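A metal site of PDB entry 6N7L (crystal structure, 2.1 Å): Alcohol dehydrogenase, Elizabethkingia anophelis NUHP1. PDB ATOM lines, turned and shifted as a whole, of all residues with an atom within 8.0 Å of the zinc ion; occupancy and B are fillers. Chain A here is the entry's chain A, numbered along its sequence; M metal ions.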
ATOM      1  N   SER A 102      -8.777  20.929 -12.783  1.00  0.00           N
ATOM      2  CA  SER A 102      -8.284  20.809 -14.154  1.00  0.00           C
ATOM      3  C   SER A 102      -7.355  19.607 -14.241  1.00  0.00           C
ATOM      4  O   SER A 102      -6.786  19.183 -13.231  1.00  0.00           O
ATOM      5  CB  SER A 102      -7.567  22.075 -14.617  1.00  0.00           C
ATOM      6  OG  SER A 102      -6.314  22.168 -13.969  1.00  0.00           O
ATOM      7  N   ALA A 103      -7.230  19.043 -15.441  1.00  0.00           N
ATOM      8  CA  ALA A 103      -6.291  17.948 -15.689  1.00  0.00           C
ATOM      9  C   ALA A 103      -5.690  18.147 -17.079  1.00  0.00           C
ATOM     10  O   ALA A 103      -6.162  18.974 -17.862  1.00  0.00           O
ATOM     11  CB  ALA A 103      -6.989  16.579 -15.551  1.00  0.00           C
ATOM     12  N   CYS A 104      -4.597  17.441 -17.364  1.00  0.00           N
ATOM     13  CA  CYS A 104      -3.882  17.741 -18.609  1.00  0.00           C
ATOM     14  C   CYS A 104      -4.614  17.218 -19.846  1.00  0.00           C
ATOM     15  O   CYS A 104      -4.494  17.812 -20.929  1.00  0.00           O
ATOM     16  CB  CYS A 104      -2.459  17.229 -18.510  1.00  0.00           C
ATOM     17  SG  CYS A 104      -2.325  15.503 -18.934  1.00  0.00           S
ATOM     18  N   GLY A 105      -5.334  16.089 -19.766  1.00  0.00           N
ATOM     19  CA  GLY A 105      -6.045  15.554 -20.918  1.00  0.00           C
ATOM     20  C   GLY A 105      -5.211  14.765 -21.913  1.00  0.00           C
ATOM     21  O   GLY A 105      -5.756  14.307 -22.944  1.00  0.00           O
ATOM     22  N   CYS A 106      -3.937  14.599 -21.672  1.00  0.00           N
ATOM     23  CA  CYS A 106      -3.085  13.955 -22.650  1.00  0.00           C
ATOM     24  C   CYS A 106      -2.086  12.959 -22.046  1.00  0.00           C
ATOM     25  O   CYS A 106      -1.210  12.470 -22.773  1.00  0.00           O
ATOM     26  CB  CYS A 106      -2.456  15.083 -23.543  1.00  0.00           C
ATOM     27  SG  CYS A 106      -1.318  16.217 -22.784  1.00  0.00           S
ATOM     28  N   CYS A 107      -2.160  12.660 -20.747  1.00  0.00           N
ATOM     29  CA  CYS A 107      -1.284  11.661 -20.105  1.00  0.00           C
ATOM     30  C   CYS A 107      -1.909  10.260 -20.072  1.00  0.00           C
ATOM     31  O   CYS A 107      -3.093  10.071 -20.367  1.00  0.00           O
ATOM     32  CB  CYS A 107      -0.901  12.106 -18.690  1.00  0.00           C
ATOM     33  SG  CYS A 107      -2.233  11.982 -17.487  1.00  0.00           S
ATOM     34  N   ASP A 108      -1.087   9.278 -19.696  1.00  0.00           N
ATOM     35  CA  ASP A 108      -1.547   7.900 -19.472  1.00  0.00           C
ATOM     36  C   ASP A 108      -2.856   7.853 -18.680  1.00  0.00           C
ATOM     37  O   ASP A 108      -3.778   7.111 -19.022  1.00  0.00           O
ATOM     38  CB  ASP A 108      -0.485   7.107 -18.699  1.00  0.00           C
ATOM     39  CG  ASP A 108       0.743   6.767 -19.536  1.00  0.00           C
ATOM     40  OD1 ASP A 108       0.762   7.042 -20.752  1.00  0.00           O
ATOM     41  OD2 ASP A 108       1.693   6.203 -18.949  1.00  0.00           O
ATOM     42  N   TYR A 109      -2.944   8.641 -17.614  1.00  0.00           N
ATOM     43  CA  TYR A 109      -4.114   8.530 -16.755  1.00  0.00           C
ATOM     44  C   TYR A 109      -5.345   9.203 -17.366  1.00  0.00           C
ATOM     45  O   TYR A 109      -6.440   8.642 -17.339  1.00  0.00           O
ATOM     46  CB  TYR A 109      -3.788   9.083 -15.369  1.00  0.00           C
ATOM     47  CG  TYR A 109      -2.672   8.289 -14.728  1.00  0.00           C
ATOM     48  CD1 TYR A 109      -2.893   6.980 -14.313  1.00  0.00           C
ATOM     49  CD2 TYR A 109      -1.397   8.813 -14.613  1.00  0.00           C
ATOM     50  CE1 TYR A 109      -1.866   6.227 -13.764  1.00  0.00           C
ATOM     51  CE2 TYR A 109      -0.371   8.078 -14.073  1.00  0.00           C
ATOM     52  CZ  TYR A 109      -0.608   6.792 -13.658  1.00  0.00           C
ATOM     53  OH  TYR A 109       0.419   6.065 -13.123  1.00  0.00           O
ATOM     54  N   CYS A 110      -5.181  10.385 -17.957  1.00  0.00           N
ATOM     55  CA  CYS A 110      -6.335  11.062 -18.561  1.00  0.00           C
ATOM     56  C   CYS A 110      -6.881  10.245 -19.738  1.00  0.00           C
ATOM     57  O   CYS A 110      -8.105  10.129 -19.893  1.00  0.00           O
ATOM     58  CB  CYS A 110      -5.946  12.480 -19.010  1.00  0.00           C
ATOM     59  SG  CYS A 110      -5.555  13.700 -17.689  1.00  0.00           S
ATOM     60  N   ILE A 111      -6.005   9.642 -20.552  1.00  0.00           N
ATOM     61  CA  ILE A 111      -6.425   8.919 -21.765  1.00  0.00           C
ATOM     62  C   ILE A 111      -7.124   7.599 -21.449  1.00  0.00           C
ATOM     63  O   ILE A 111      -7.953   7.127 -22.222  1.00  0.00           O
ATOM     64  CB  ILE A 111      -5.198   8.721 -22.677  1.00  0.00           C
ATOM     65  CG1 ILE A 111      -4.723  10.072 -23.209  1.00  0.00           C
ATOM     66  CG2 ILE A 111      -5.513   7.758 -23.853  1.00  0.00           C
ATOM     67  CD1 ILE A 111      -3.352  10.020 -23.845  1.00  0.00           C
ATOM     68  N   TRP A 114      -8.767   7.682 -16.226  1.00  0.00           N
ATOM     69  CA  TRP A 114      -8.370   7.899 -14.835  1.00  0.00           C
ATOM     70  C   TRP A 114      -7.821   9.310 -14.613  1.00  0.00           C
ATOM     71  O   TRP A 114      -6.805   9.490 -13.946  1.00  0.00           O
ATOM     72  CB  TRP A 114      -7.337   6.836 -14.423  1.00  0.00           C
ATOM     73  CG  TRP A 114      -7.997   5.546 -14.179  1.00  0.00           C
ATOM     74  CD1 TRP A 114      -8.121   4.509 -15.051  1.00  0.00           C
ATOM     75  CD2 TRP A 114      -8.722   5.187 -13.003  1.00  0.00           C
ATOM     76  NE1 TRP A 114      -8.864   3.504 -14.478  1.00  0.00           N
ATOM     77  CE2 TRP A 114      -9.248   3.892 -13.222  1.00  0.00           C
ATOM     78  CE3 TRP A 114      -8.981   5.810 -11.776  1.00  0.00           C
ATOM     79  CZ2 TRP A 114     -10.001   3.216 -12.262  1.00  0.00           C
ATOM     80  CZ3 TRP A 114      -9.735   5.143 -10.820  1.00  0.00           C
ATOM     81  CH2 TRP A 114     -10.236   3.866 -11.068  1.00  0.00           C
ATOM     82  N   GLU A 115      -8.524  10.322 -15.148  1.00  0.00           N
ATOM     83  CA  GLU A 115      -8.040  11.694 -15.020  1.00  0.00           C
ATOM     84  C   GLU A 115      -7.949  12.159 -13.561  1.00  0.00           C
ATOM     85  O   GLU A 115      -7.262  13.142 -13.295  1.00  0.00           O
ATOM     86  CB  GLU A 115      -8.930  12.659 -15.811  1.00  0.00           C
ATOM     87  CG  GLU A 115     -10.414  12.580 -15.508  1.00  0.00           C
ATOM     88  CD  GLU A 115     -11.266  13.435 -16.444  1.00  0.00           C
ATOM     89  OE1 GLU A 115     -12.445  13.643 -16.115  1.00  0.00           O
ATOM     90  OE2 GLU A 115     -10.748  13.902 -17.497  1.00  0.00           O
ATOM     91  N   THR A 116      -8.625  11.471 -12.625  1.00  0.00           N
ATOM     92  CA  THR A 116      -8.429  11.758 -11.204  1.00  0.00           C
ATOM     93  C   THR A 116      -7.005  11.514 -10.748  1.00  0.00           C
ATOM     94  O   THR A 116      -6.621  11.993  -9.676  1.00  0.00           O
ATOM     95  CB  THR A 116      -9.372  10.908 -10.336  1.00  0.00           C
ATOM     96  OG1 THR A 116      -9.252   9.540 -10.723  1.00  0.00           O
ATOM     97  CG2 THR A 116     -10.810  11.347 -10.507  1.00  0.00           C
ATOM     98  N   LEU A 117      -6.217  10.766 -11.515  1.00  0.00           N
ATOM     99  CA  LEU A 117      -4.842  10.479 -11.161  1.00  0.00           C
ATOM    100  C   LEU A 117      -3.839  11.337 -11.930  1.00  0.00           C
ATOM    101  O   LEU A 117      -2.625  11.120 -11.806  1.00  0.00           O
ATOM    102  CB  LEU A 117      -4.531   8.995 -11.385  1.00  0.00           C
ATOM    103  CG  LEU A 117      -5.494   8.035 -10.660  1.00  0.00           C
ATOM    104  CD1 LEU A 117      -5.121   6.580 -10.917  1.00  0.00           C
ATOM    105  CD2 LEU A 117      -5.468   8.345  -9.151  1.00  0.00           C
ATOM    106  N   CYS A 118      -4.312  12.287 -12.736  1.00  0.00           N
ATOM    107  CA  CYS A 118      -3.414  13.112 -13.545  1.00  0.00           C
ATOM    108  C   CYS A 118      -2.416  13.822 -12.645  1.00  0.00           C
ATOM    109  O   CYS A 118      -2.799  14.498 -11.679  1.00  0.00           O
ATOM    110  CB  CYS A 118      -4.212  14.146 -14.358  1.00  0.00           C
ATOM    111  SG  CYS A 118      -3.202  15.261 -15.391  1.00  0.00           S
ATOM    112  N   GLU A 119      -1.131  13.638 -12.930  1.00  0.00           N
ATOM    113  CA  GLU A 119      -0.093  14.247 -12.115  1.00  0.00           C
ATOM    114  C   GLU A 119       0.072  15.733 -12.408  1.00  0.00           C
ATOM    115  O   GLU A 119       0.741  16.420 -11.632  1.00  0.00           O
ATOM    116  CB  GLU A 119       1.228  13.497 -12.315  1.00  0.00           C
ATOM    117  CG  GLU A 119       1.183  12.094 -11.695  1.00  0.00           C
ATOM    118  CD  GLU A 119       2.501  11.358 -11.763  1.00  0.00           C
ATOM    119  OE1 GLU A 119       3.457  11.887 -12.362  1.00  0.00           O
ATOM    120  OE2 GLU A 119       2.578  10.232 -11.219  1.00  0.00           O
ATOM    121  N   ALA A 120      -0.525  16.242 -13.470  1.00  0.00           N
ATOM    122  CA  ALA A 120      -0.513  17.676 -13.731  1.00  0.00           C
ATOM    123  C   ALA A 120      -1.814  18.348 -13.314  1.00  0.00           C
ATOM    124  O   ALA A 120      -2.075  19.484 -13.728  1.00  0.00           O
ATOM    125  CB  ALA A 120      -0.221  17.938 -15.211  1.00  0.00           C
ATOM    126  N   GLN A 121      -2.640  17.674 -12.519  1.00  0.00           N
ATOM    127  CA  GLN A 121      -3.926  18.261 -12.136  1.00  0.00           C
ATOM    128  C   GLN A 121      -3.736  19.453 -11.207  1.00  0.00           C
ATOM    129  O   GLN A 121      -2.716  19.583 -10.528  1.00  0.00           O
ATOM    130  CB  GLN A 121      -4.794  17.222 -11.453  1.00  0.00           C
ATOM    131  CG  GLN A 121      -4.352  16.804 -10.067  1.00  0.00           C
ATOM    132  CD  GLN A 121      -5.243  15.689  -9.529  1.00  0.00           C
ATOM    133  OE1 GLN A 121      -6.076  15.926  -8.659  1.00  0.00           O
ATOM    134  NE2 GLN A 121      -5.091  14.480 -10.066  1.00  0.00           N
ATOM    135  N   TYR A 142     -13.702  21.344 -16.777  1.00  0.00           N
ATOM    136  CA  TYR A 142     -13.795  20.364 -15.697  1.00  0.00           C
ATOM    137  C   TYR A 142     -14.874  20.706 -14.687  1.00  0.00           C
ATOM    138  O   TYR A 142     -14.973  20.023 -13.666  1.00  0.00           O
ATOM    139  CB  TYR A 142     -12.429  20.197 -15.008  1.00  0.00           C
ATOM    140  CG  TYR A 142     -11.447  19.517 -15.928  1.00  0.00           C
ATOM    141  CD1 TYR A 142     -10.713  20.248 -16.849  1.00  0.00           C
ATOM    142  CD2 TYR A 142     -11.290  18.134 -15.916  1.00  0.00           C
ATOM    143  CE1 TYR A 142      -9.832  19.624 -17.725  1.00  0.00           C
ATOM    144  CE2 TYR A 142     -10.414  17.507 -16.799  1.00  0.00           C
ATOM    145  CZ  TYR A 142      -9.686  18.259 -17.699  1.00  0.00           C
ATOM    146  OH  TYR A 142      -8.807  17.651 -18.568  1.00  0.00           O
HETATM  147 ZN    ZN M   1      -3.314  14.130 -17.426  1.00  0.00          ZN
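N of Cys 106 lies close to SG of Cys 104 (3.3 Å).
SG of Cys 110 lies close to N of Gly 105 (3.2 Å).
The side-chain sulfur (SG) of Cys 118 sits close to the backbone NH (N) of Ala 120 (3.4 Å).
The side-chain amide nitrogen (NE2) of Gln 121 sits at hydrogen-bond distance from the backbone carbonyl oxygen (O) of Cys 118 (2.8 Å).
The side-chain sulfur (SG) of Cys 107 lies close to the backbone NH (N) of Tyr 109.
Residues that only touch the zinc ion: Gly 105 (3.7 Å).
Within 4 Å of the zinc ion: Cys 104, Gly 105, Cys 107, Cys 110 and Cys 118.
The zinc ion is bound by SG of Cys 104, at 2.3 Å.
The side-chain sulfur (SG) of Cys 110 binds the zinc ion, 2.3 Å away.
SG of Cys 118 is bound to the zinc ion (2.3 Å).
SG of Cys 107 is bound to the zinc ion.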
